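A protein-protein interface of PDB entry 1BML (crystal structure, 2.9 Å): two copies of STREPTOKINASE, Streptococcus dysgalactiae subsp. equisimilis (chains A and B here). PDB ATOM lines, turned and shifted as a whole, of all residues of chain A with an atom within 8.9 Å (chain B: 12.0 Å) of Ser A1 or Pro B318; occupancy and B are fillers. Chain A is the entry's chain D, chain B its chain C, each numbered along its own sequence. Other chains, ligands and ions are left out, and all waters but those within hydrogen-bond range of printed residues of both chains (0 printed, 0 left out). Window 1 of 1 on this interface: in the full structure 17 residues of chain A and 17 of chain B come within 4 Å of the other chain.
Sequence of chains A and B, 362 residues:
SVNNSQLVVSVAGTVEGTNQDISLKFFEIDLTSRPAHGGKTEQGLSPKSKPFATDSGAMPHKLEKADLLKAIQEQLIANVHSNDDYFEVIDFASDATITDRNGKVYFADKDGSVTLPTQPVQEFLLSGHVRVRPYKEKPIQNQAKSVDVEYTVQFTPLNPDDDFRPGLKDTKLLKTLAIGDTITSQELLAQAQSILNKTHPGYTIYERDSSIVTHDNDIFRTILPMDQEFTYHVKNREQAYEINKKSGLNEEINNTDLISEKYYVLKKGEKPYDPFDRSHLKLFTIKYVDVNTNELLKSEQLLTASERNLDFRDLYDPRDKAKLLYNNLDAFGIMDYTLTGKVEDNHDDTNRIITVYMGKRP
O of Asp B311 is in hydrogen-bond range of N of Leu B324, at 3.5 Å.
NH1 of Arg B313 sits at hydrogen-bond distance from O of Lys B323 (3.2 Å).
The backbone NH (N) of Asp B314 lies within hydrogen-bond range of the side-chain carboxylate (OD2) of Asp B320, 2.5 Å away.
OD2 of Asp B317 lies within salt-bridge range of NH1 of Arg B319 (3.1 Å).
The side-chain carboxylate of Asp B320 lies within salt-bridge range of the side-chain amino group of Lys B323 (3.2 Å).
The backbone carbonyl oxygen (O) of Ser A1 lies close to the side-chain amide oxygen (OD1) of Asn A3 (3.3 Å).
Val A2 touches just one residue of chain B: Arg B319.
Of chain B, only Pro B318 comes within 4 Å of Asn A3.
Printed residues of chain B within 4 Å of Arg A101: Asp B311, Phe B312, Asp B320 and Lys B323.
Pro B318 touches just these residues of chain A: Ser A1 (3.96 Å) and Asn A3 (3.2 Å).
Of the printed residues of chain A, Asp B320 touches Arg A101 (3.0 Å).
Asn B327 touches none of the printed residues of chain A.
OD2 of Asp B311 is in salt-bridge range of NH1 of Arg A101, at 3.8 Å.
The backbone carbonyl oxygen (O) of Phe B312 lies within hydrogen-bond range of the guanidinium group (NH2) of Arg A101 (3.5 Å).
O of Pro B318 is in hydrogen-bond range of ND2 of Asn A3 (3.2 Å).
The guanidinium group (NH2) of Arg B319 sits close to the side-chain amide nitrogen (NE2) of Gln A6 (3.4 Å).
NH2 of Arg B319 lies within salt-bridge range of OE1 of Glu A123, at 3.3 Å.
OD2 of Asp B320 is in salt-bridge range of NH2 of Arg A101 (3.0 Å).
NZ of Lys B323 sits at hydrogen-bond distance from O of Val A121, 2.6 Å away.
No position is printed for both chains.
Of the 12 pairs that touch across the chains among the printed residues, none has its exchanged pair printed and touching as well.
Of the 17 printed residues of chain B, 6 touch a printed residue of chain A.
Hydrophobic or aromatic side chains of chain B within 4 Å of the printed part of chain A: Pro B318.
Of the 13 printed residues of chain A, 7 touch a printed residue of chain B.
Hydrophobic or aromatic side chains of chain A that line the printed part of chain B: Val A121.
Along chain A the printed residues that touch a printed residue of chain B span positions 1 to 123.
Among the printed residues, 12 pairs touch across the chains.
Among the printed residues, Asp or Glu carboxylates within 4 Å of a Lys or Arg side-chain nitrogen of the other chain: Arg A101 with Asp B311, Arg A101 with Asp B320 and Glu A123 with Arg B319.
N of Ser A1 touches CG of Pro B318, 3.96 Å away.
Arg B319 touches Ser A1.
Arg B319 touches Val A2 (NE to O, 3.9 Å).
Arg A101 touches Lys B323 (NH1 to CE, 3.7 Å).
CG1 of Val A121 touches CB of Arg B319, at 3.7 Å.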
ATOM      1  N   SER A   1      -5.084  22.797  12.508  1.00  0.00           N
ATOM      2  CA  SER A   1      -5.364  21.548  11.810  1.00  0.00           C
ATOM      3  C   SER A   1      -6.348  20.671  12.585  1.00  0.00           C
ATOM      4  O   SER A   1      -6.862  21.081  13.633  1.00  0.00           O
ATOM      5  CB  SER A   1      -4.058  20.784  11.574  1.00  0.00           C
ATOM      6  OG  SER A   1      -3.116  21.591  10.885  1.00  0.00           O
ATOM      7  N   VAL A   2      -6.601  19.467  12.065  1.00  0.00           N
ATOM      8  CA  VAL A   2      -7.528  18.518  12.689  1.00  0.00           C
ATOM      9  C   VAL A   2      -7.443  18.592  14.211  1.00  0.00           C
ATOM     10  O   VAL A   2      -6.396  18.293  14.795  1.00  0.00           O
ATOM     11  CB  VAL A   2      -7.237  17.055  12.243  1.00  0.00           C
ATOM     12  CG1 VAL A   2      -8.414  16.153  12.607  1.00  0.00           C
ATOM     13  CG2 VAL A   2      -6.975  17.007  10.748  1.00  0.00           C
ATOM     14  N   ASN A   3      -8.541  19.017  14.837  1.00  0.00           N
ATOM     15  CA  ASN A   3      -8.620  19.133  16.292  1.00  0.00           C
ATOM     16  C   ASN A   3      -8.538  17.759  16.940  1.00  0.00           C
ATOM     17  O   ASN A   3      -9.447  17.332  17.661  1.00  0.00           O
ATOM     18  CB  ASN A   3      -9.927  19.809  16.701  1.00  0.00           C
ATOM     19  CG  ASN A   3      -9.816  21.309  16.710  1.00  0.00           C
ATOM     20  OD1 ASN A   3      -8.973  21.874  16.019  1.00  0.00           O
ATOM     21  ND2 ASN A   3     -10.666  21.967  17.495  1.00  0.00           N
ATOM     22  N   ASN A   4      -7.431  17.076  16.677  1.00  0.00           N
ATOM     23  CA  ASN A   4      -7.192  15.754  17.203  1.00  0.00           C
ATOM     24  C   ASN A   4      -5.704  15.540  17.232  1.00  0.00           C
ATOM     25  O   ASN A   4      -4.974  16.049  16.386  1.00  0.00           O
ATOM     26  CB  ASN A   4      -7.833  14.694  16.319  1.00  0.00           C
ATOM     27  CG  ASN A   4      -7.629  13.297  16.860  1.00  0.00           C
ATOM     28  OD1 ASN A   4      -7.826  12.312  16.150  1.00  0.00           O
ATOM     29  ND2 ASN A   4      -7.230  13.202  18.126  1.00  0.00           N
ATOM     30  N   SER A   5      -5.255  14.779  18.211  1.00  0.00           N
ATOM     31  CA  SER A   5      -3.847  14.510  18.345  1.00  0.00           C
ATOM     32  C   SER A   5      -3.332  13.543  17.293  1.00  0.00           C
ATOM     33  O   SER A   5      -3.872  12.450  17.079  1.00  0.00           O
ATOM     34  CB  SER A   5      -3.550  13.983  19.749  1.00  0.00           C
ATOM     35  OG  SER A   5      -3.159  15.054  20.601  1.00  0.00           O
ATOM     36  N   GLN A   6      -2.271  13.979  16.635  1.00  0.00           N
ATOM     37  CA  GLN A   6      -1.621  13.199  15.604  1.00  0.00           C
ATOM     38  C   GLN A   6      -0.116  13.286  15.826  1.00  0.00           C
ATOM     39  O   GLN A   6       0.392  14.253  16.406  1.00  0.00           O
ATOM     40  CB  GLN A   6      -1.975  13.751  14.228  1.00  0.00           C
ATOM     41  CG  GLN A   6      -1.530  15.181  14.027  1.00  0.00           C
ATOM     42  CD  GLN A   6      -2.337  15.898  12.972  1.00  0.00           C
ATOM     43  OE1 GLN A   6      -2.983  15.268  12.133  1.00  0.00           O
ATOM     44  NE2 GLN A   6      -2.307  17.223  13.006  1.00  0.00           N
ATOM     45  N   VAL A   8       3.505  13.593  14.161  1.00  0.00           N
ATOM     46  CA  VAL A   8       4.253  13.988  12.983  1.00  0.00           C
ATOM     47  C   VAL A   8       5.533  13.149  12.917  1.00  0.00           C
ATOM     48  O   VAL A   8       6.459  13.331  13.724  1.00  0.00           O
ATOM     49  CB  VAL A   8       4.664  15.449  13.083  1.00  0.00           C
ATOM     50  CG1 VAL A   8       5.313  15.907  11.795  1.00  0.00           C
ATOM     51  CG2 VAL A   8       3.465  16.273  13.415  1.00  0.00           C
ATOM     52  N   GLU A  28       1.754  12.589   8.806  1.00  0.00           N
ATOM     53  CA  GLU A  28       1.084  12.552  10.086  1.00  0.00           C
ATOM     54  C   GLU A  28       0.319  11.278  10.329  1.00  0.00           C
ATOM     55  O   GLU A  28      -0.329  10.737   9.433  1.00  0.00           O
ATOM     56  CB  GLU A  28       0.131  13.735  10.207  1.00  0.00           C
ATOM     57  CG  GLU A  28       0.050  14.600   8.970  1.00  0.00           C
ATOM     58  CD  GLU A  28       0.790  15.898   9.143  1.00  0.00           C
ATOM     59  OE1 GLU A  28       1.779  15.908   9.895  1.00  0.00           O
ATOM     60  OE2 GLU A  28       0.390  16.910   8.535  1.00  0.00           O
ATOM     61  N   ASP A  30      -2.616   9.618  12.799  1.00  0.00           N
ATOM     62  CA  ASP A  30      -3.638  10.115  13.691  1.00  0.00           C
ATOM     63  C   ASP A  30      -3.843   9.263  14.919  1.00  0.00           C
ATOM     64  O   ASP A  30      -4.095   8.057  14.846  1.00  0.00           O
ATOM     65  CB  ASP A  30      -4.966  10.321  12.975  1.00  0.00           C
ATOM     66  CG  ASP A  30      -5.651  11.599  13.415  1.00  0.00           C
ATOM     67  OD1 ASP A  30      -5.198  12.199  14.419  1.00  0.00           O
ATOM     68  OD2 ASP A  30      -6.630  12.010  12.762  1.00  0.00           O
ATOM     69  N   ARG A 101       5.092  19.086  22.671  1.00  0.00           N
ATOM     70  CA  ARG A 101       5.396  20.496  22.494  1.00  0.00           C
ATOM     71  C   ARG A 101       6.491  21.042  23.389  1.00  0.00           C
ATOM     72  O   ARG A 101       7.283  21.885  22.959  1.00  0.00           O
ATOM     73  CB  ARG A 101       4.131  21.346  22.678  1.00  0.00           C
ATOM     74  CG  ARG A 101       4.347  22.813  22.338  1.00  0.00           C
ATOM     75  CD  ARG A 101       3.722  23.747  23.369  1.00  0.00           C
ATOM     76  NE  ARG A 101       2.647  24.543  22.771  1.00  0.00           N
ATOM     77  CZ  ARG A 101       1.359  24.212  22.821  1.00  0.00           C
ATOM     78  NH1 ARG A 101       0.984  23.099  23.450  1.00  0.00           N
ATOM     79  NH2 ARG A 101       0.446  24.974  22.217  1.00  0.00           N
ATOM     80  N   VAL A 121      -4.395  17.226  23.997  1.00  0.00           N
ATOM     81  CA  VAL A 121      -4.451  17.658  22.578  1.00  0.00           C
ATOM     82  C   VAL A 121      -3.465  18.657  21.999  1.00  0.00           C
ATOM     83  O   VAL A 121      -3.575  19.881  22.180  1.00  0.00           O
ATOM     84  CB  VAL A 121      -5.831  18.135  22.172  1.00  0.00           C
ATOM     85  CG1 VAL A 121      -5.774  18.767  20.770  1.00  0.00           C
ATOM     86  CG2 VAL A 121      -6.768  16.941  22.157  1.00  0.00           C
ATOM     87  N   GLN A 122      -2.519  18.090  21.255  1.00  0.00           N
ATOM     88  CA  GLN A 122      -1.440  18.831  20.614  1.00  0.00           C
ATOM     89  C   GLN A 122      -0.886  17.875  19.578  1.00  0.00           C
ATOM     90  O   GLN A 122      -1.483  16.832  19.322  1.00  0.00           O
ATOM     91  CB  GLN A 122      -0.345  19.147  21.641  1.00  0.00           C
ATOM     92  CG  GLN A 122       0.522  17.934  21.977  1.00  0.00           C
ATOM     93  CD  GLN A 122       0.701  17.699  23.458  1.00  0.00           C
ATOM     94  OE1 GLN A 122      -0.143  17.061  24.111  1.00  0.00           O
ATOM     95  NE2 GLN A 122       1.817  18.200  24.005  1.00  0.00           N
ATOM     96  N   GLU A 123       0.247  18.218  18.980  1.00  0.00           N
ATOM     97  CA  GLU A 123       0.834  17.303  18.020  1.00  0.00           C
ATOM     98  C   GLU A 123       2.186  16.834  18.533  1.00  0.00           C
ATOM     99  O   GLU A 123       2.950  17.613  19.127  1.00  0.00           O
ATOM    100  CB  GLU A 123       0.973  17.962  16.645  1.00  0.00           C
ATOM    101  CG  GLU A 123       2.032  19.042  16.530  1.00  0.00           C
ATOM    102  CD  GLU A 123       2.228  19.421  15.079  1.00  0.00           C
ATOM    103  OE1 GLU A 123       1.427  18.879  14.271  1.00  0.00           O
ATOM    104  OE2 GLU A 123       3.143  20.237  14.755  1.00  0.00           O
ATOM    105  N   ASN B 309      -4.881  20.657  30.852  1.00  0.00           N
ATOM    106  CA  ASN B 309      -5.044  21.914  30.115  1.00  0.00           C
ATOM    107  C   ASN B 309      -4.181  23.045  30.599  1.00  0.00           C
ATOM    108  O   ASN B 309      -4.133  24.110  29.976  1.00  0.00           O
ATOM    109  CB  ASN B 309      -6.484  22.381  30.175  1.00  0.00           C
ATOM    110  CG  ASN B 309      -7.449  21.368  29.626  1.00  0.00           C
ATOM    111  OD1 ASN B 309      -8.645  21.604  29.643  1.00  0.00           O
ATOM    112  ND2 ASN B 309      -6.946  20.229  29.138  1.00  0.00           N
ATOM    113  N   ASP B 311      -1.522  24.582  30.257  1.00  0.00           N
ATOM    114  CA  ASP B 311      -0.467  24.623  29.266  1.00  0.00           C
ATOM    115  C   ASP B 311      -0.663  25.903  28.485  1.00  0.00           C
ATOM    116  O   ASP B 311      -1.762  26.465  28.458  1.00  0.00           O
ATOM    117  CB  ASP B 311      -0.604  23.422  28.337  1.00  0.00           C
ATOM    118  CG  ASP B 311       0.661  23.120  27.592  1.00  0.00           C
ATOM    119  OD1 ASP B 311       1.522  24.017  27.522  1.00  0.00           O
ATOM    120  OD2 ASP B 311       0.797  21.987  27.076  1.00  0.00           O
ATOM    121  N   PHE B 312       0.401  26.372  27.853  1.00  0.00           N
ATOM    122  CA  PHE B 312       0.307  27.582  27.054  1.00  0.00           C
ATOM    123  C   PHE B 312      -0.558  27.333  25.835  1.00  0.00           C
ATOM    124  O   PHE B 312      -0.622  26.226  25.292  1.00  0.00           O
ATOM    125  CB  PHE B 312       1.683  28.035  26.621  1.00  0.00           C
ATOM    126  CG  PHE B 312       2.700  27.888  27.687  1.00  0.00           C
ATOM    127  CD1 PHE B 312       3.267  26.643  27.950  1.00  0.00           C
ATOM    128  CD2 PHE B 312       3.092  28.980  28.440  1.00  0.00           C
ATOM    129  CE1 PHE B 312       4.214  26.487  28.946  1.00  0.00           C
ATOM    130  CE2 PHE B 312       4.039  28.839  29.436  1.00  0.00           C
ATOM    131  CZ  PHE B 312       4.603  27.585  29.690  1.00  0.00           C
ATOM    132  N   ARG B 313      -1.204  28.403  25.400  1.00  0.00           N
ATOM    133  CA  ARG B 313      -2.104  28.343  24.282  1.00  0.00           C
ATOM    134  C   ARG B 313      -1.780  29.432  23.296  1.00  0.00           C
ATOM    135  O   ARG B 313      -1.607  30.603  23.656  1.00  0.00           O
ATOM    136  CB  ARG B 313      -3.556  28.471  24.771  1.00  0.00           C
ATOM    137  CG  ARG B 313      -4.406  29.484  24.045  1.00  0.00           C
ATOM    138  CD  ARG B 313      -5.642  29.775  24.854  1.00  0.00           C
ATOM    139  NE  ARG B 313      -6.798  30.167  24.050  1.00  0.00           N
ATOM    140  CZ  ARG B 313      -8.057  29.894  24.380  1.00  0.00           C
ATOM    141  NH1 ARG B 313      -8.316  29.228  25.497  1.00  0.00           N
ATOM    142  NH2 ARG B 313      -9.062  30.293  23.609  1.00  0.00           N
ATOM    143  N   ASP B 314      -1.680  28.992  22.046  1.00  0.00           N
ATOM    144  CA  ASP B 314      -1.421  29.824  20.897  1.00  0.00           C
ATOM    145  C   ASP B 314      -2.801  30.226  20.362  1.00  0.00           C
ATOM    146  O   ASP B 314      -3.649  29.379  20.039  1.00  0.00           O
ATOM    147  CB  ASP B 314      -0.667  29.013  19.845  1.00  0.00           C
ATOM    148  CG  ASP B 314      -0.556  29.736  18.515  1.00  0.00           C
ATOM    149  OD1 ASP B 314      -0.868  30.948  18.455  1.00  0.00           O
ATOM    150  OD2 ASP B 314      -0.154  29.085  17.536  1.00  0.00           O
ATOM    151  N   LEU B 315      -3.017  31.526  20.257  1.00  0.00           N
ATOM    152  CA  LEU B 315      -4.300  32.007  19.800  1.00  0.00           C
ATOM    153  C   LEU B 315      -4.537  31.877  18.298  1.00  0.00           C
ATOM    154  O   LEU B 315      -5.426  32.519  17.753  1.00  0.00           O
ATOM    155  CB  LEU B 315      -4.483  33.456  20.240  1.00  0.00           C
ATOM    156  CG  LEU B 315      -5.009  33.635  21.664  1.00  0.00           C
ATOM    157  CD1 LEU B 315      -5.406  35.075  21.858  1.00  0.00           C
ATOM    158  CD2 LEU B 315      -6.197  32.732  21.905  1.00  0.00           C
ATOM    159  N   TYR B 316      -3.749  31.048  17.626  1.00  0.00           N
ATOM    160  CA  TYR B 316      -3.923  30.853  16.195  1.00  0.00           C
ATOM    161  C   TYR B 316      -4.253  29.401  16.000  1.00  0.00           C
ATOM    162  O   TYR B 316      -4.994  29.018  15.090  1.00  0.00           O
ATOM    163  CB  TYR B 316      -2.641  31.109  15.486  1.00  0.00           C
ATOM    164  CG  TYR B 316      -2.315  32.540  15.246  1.00  0.00           C
ATOM    165  CD1 TYR B 316      -2.819  33.209  14.137  1.00  0.00           C
ATOM    166  CD2 TYR B 316      -1.381  33.187  16.030  1.00  0.00           C
ATOM    167  CE1 TYR B 316      -2.373  34.459  13.815  1.00  0.00           C
ATOM    168  CE2 TYR B 316      -0.930  34.430  15.718  1.00  0.00           C
ATOM    169  CZ  TYR B 316      -1.427  35.058  14.612  1.00  0.00           C
ATOM    170  OH  TYR B 316      -0.923  36.282  14.265  1.00  0.00           O
ATOM    171  N   ASP B 317      -3.679  28.602  16.885  1.00  0.00           N
ATOM    172  CA  ASP B 317      -3.831  27.171  16.861  1.00  0.00           C
ATOM    173  C   ASP B 317      -5.148  26.743  17.511  1.00  0.00           C
ATOM    174  O   ASP B 317      -5.359  26.931  18.714  1.00  0.00           O
ATOM    175  CB  ASP B 317      -2.635  26.565  17.585  1.00  0.00           C
ATOM    176  CG  ASP B 317      -2.493  25.097  17.340  1.00  0.00           C
ATOM    177  OD1 ASP B 317      -3.533  24.412  17.211  1.00  0.00           O
ATOM    178  OD2 ASP B 317      -1.338  24.628  17.283  1.00  0.00           O
ATOM    179  N   PRO B 318      -6.067  26.190  16.710  1.00  0.00           N
ATOM    180  CA  PRO B 318      -7.375  25.723  17.185  1.00  0.00           C
ATOM    181  C   PRO B 318      -7.383  24.517  18.118  1.00  0.00           C
ATOM    182  O   PRO B 318      -8.459  24.024  18.454  1.00  0.00           O
ATOM    183  CB  PRO B 318      -8.153  25.455  15.905  1.00  0.00           C
ATOM    184  CG  PRO B 318      -7.120  25.225  14.881  1.00  0.00           C
ATOM    185  CD  PRO B 318      -5.929  26.051  15.252  1.00  0.00           C
ATOM    186  N   ARG B 319      -6.215  24.025  18.535  1.00  0.00           N
ATOM    187  CA  ARG B 319      -6.163  22.884  19.475  1.00  0.00           C
ATOM    188  C   ARG B 319      -5.952  23.464  20.873  1.00  0.00           C
ATOM    189  O   ARG B 319      -6.407  22.927  21.884  1.00  0.00           O
ATOM    190  CB  ARG B 319      -5.015  21.943  19.129  1.00  0.00           C
ATOM    191  CG  ARG B 319      -5.248  21.135  17.874  1.00  0.00           C
ATOM    192  CD  ARG B 319      -4.417  21.662  16.732  1.00  0.00           C
ATOM    193  NE  ARG B 319      -3.570  20.619  16.156  1.00  0.00           N
ATOM    194  CZ  ARG B 319      -2.332  20.818  15.692  1.00  0.00           C
ATOM    195  NH1 ARG B 319      -1.772  22.034  15.726  1.00  0.00           N
ATOM    196  NH2 ARG B 319      -1.651  19.792  15.177  1.00  0.00           N
ATOM    197  N   ASP B 320      -5.266  24.594  20.893  1.00  0.00           N
ATOM    198  CA  ASP B 320      -4.981  25.341  22.101  1.00  0.00           C
ATOM    199  C   ASP B 320      -6.252  26.011  22.636  1.00  0.00           C
ATOM    200  O   ASP B 320      -6.187  27.058  23.303  1.00  0.00           O
ATOM    201  CB  ASP B 320      -3.959  26.430  21.778  1.00  0.00           C
ATOM    202  CG  ASP B 320      -2.624  25.868  21.378  1.00  0.00           C
ATOM    203  OD1 ASP B 320      -2.480  24.615  21.406  1.00  0.00           O
ATOM    204  OD2 ASP B 320      -1.725  26.681  21.041  1.00  0.00           O
ATOM    205  N   LYS B 321      -7.408  25.438  22.333  1.00  0.00           N
ATOM    206  CA  LYS B 321      -8.653  26.036  22.787  1.00  0.00           C
ATOM    207  C   LYS B 321      -8.936  25.839  24.278  1.00  0.00           C
ATOM    208  O   LYS B 321      -9.317  26.786  24.970  1.00  0.00           O
ATOM    209  CB  LYS B 321      -9.810  25.497  21.956  1.00  0.00           C
ATOM    210  CG  LYS B 321     -10.065  26.299  20.714  1.00  0.00           C
ATOM    211  CD  LYS B 321     -10.797  25.464  19.692  1.00  0.00           C
ATOM    212  CE  LYS B 321     -11.958  26.228  19.091  1.00  0.00           C
ATOM    213  NZ  LYS B 321     -12.787  25.354  18.195  1.00  0.00           N
ATOM    214  N   ALA B 322      -8.756  24.614  24.769  1.00  0.00           N
ATOM    215  CA  ALA B 322      -9.001  24.323  26.179  1.00  0.00           C
ATOM    216  C   ALA B 322      -7.789  24.636  27.045  1.00  0.00           C
ATOM    217  O   ALA B 322      -7.783  24.322  28.223  1.00  0.00           O
ATOM    218  CB  ALA B 322      -9.390  22.865  26.357  1.00  0.00           C
ATOM    219  N   LYS B 323      -6.762  25.253  26.473  1.00  0.00           N
ATOM    220  CA  LYS B 323      -5.555  25.568  27.236  1.00  0.00           C
ATOM    221  C   LYS B 323      -5.726  26.860  28.031  1.00  0.00           C
ATOM    222  O   LYS B 323      -6.389  27.800  27.574  1.00  0.00           O
ATOM    223  CB  LYS B 323      -4.359  25.676  26.286  1.00  0.00           C
ATOM    224  CG  LYS B 323      -3.541  24.402  26.192  1.00  0.00           C
ATOM    225  CD  LYS B 323      -3.908  23.574  24.980  1.00  0.00           C
ATOM    226  CE  LYS B 323      -2.673  23.328  24.104  1.00  0.00           C
ATOM    227  NZ  LYS B 323      -2.717  22.062  23.280  1.00  0.00           N
ATOM    228  N   LEU B 324      -5.120  26.931  29.210  1.00  0.00           N
ATOM    229  CA  LEU B 324      -5.290  28.130  30.026  1.00  0.00           C
ATOM    230  C   LEU B 324      -4.297  29.253  29.789  1.00  0.00           C
ATOM    231  O   LEU B 324      -4.681  30.418  29.665  1.00  0.00           O
ATOM    232  CB  LEU B 324      -5.294  27.780  31.529  1.00  0.00           C
ATOM    233  CG  LEU B 324      -6.025  26.532  32.057  1.00  0.00           C
ATOM    234  CD1 LEU B 324      -5.823  26.477  33.547  1.00  0.00           C
ATOM    235  CD2 LEU B 324      -7.517  26.552  31.754  1.00  0.00           C
ATOM    236  N   TYR B 326      -2.135  31.814  28.008  1.00  0.00           N
ATOM    237  CA  TYR B 326      -1.954  32.506  26.726  1.00  0.00           C
ATOM    238  C   TYR B 326      -0.443  32.657  26.507  1.00  0.00           C
ATOM    239  O   TYR B 326       0.328  31.828  26.964  1.00  0.00           O
ATOM    240  CB  TYR B 326      -2.599  33.895  26.762  1.00  0.00           C
ATOM    241  CG  TYR B 326      -4.090  33.872  26.956  1.00  0.00           C
ATOM    242  CD1 TYR B 326      -4.874  32.909  26.331  1.00  0.00           C
ATOM    243  CD2 TYR B 326      -4.718  34.799  27.777  1.00  0.00           C
ATOM    244  CE1 TYR B 326      -6.241  32.863  26.517  1.00  0.00           C
ATOM    245  CE2 TYR B 326      -6.098  34.762  27.974  1.00  0.00           C
ATOM    246  CZ  TYR B 326      -6.847  33.790  27.340  1.00  0.00           C
ATOM    247  OH  TYR B 326      -8.205  33.735  27.524  1.00  0.00           O
ATOM    248  N   ASN B 327      -0.025  33.697  25.796  1.00  0.00           N
ATOM    249  CA  ASN B 327       1.397  33.939  25.567  1.00  0.00           C
ATOM    250  C   ASN B 327       1.585  35.165  24.711  1.00  0.00           C
ATOM    251  O   ASN B 327       2.712  35.614  24.488  1.00  0.00           O
ATOM    252  CB  ASN B 327       2.059  32.750  24.881  1.00  0.00           C
ATOM    253  CG  ASN B 327       1.377  32.363  23.600  1.00  0.00           C
ATOM    254  OD1 ASN B 327       1.160  31.179  23.345  1.00  0.00           O
ATOM    255  ND2 ASN B 327       1.040  33.354  22.775  1.00  0.00           N
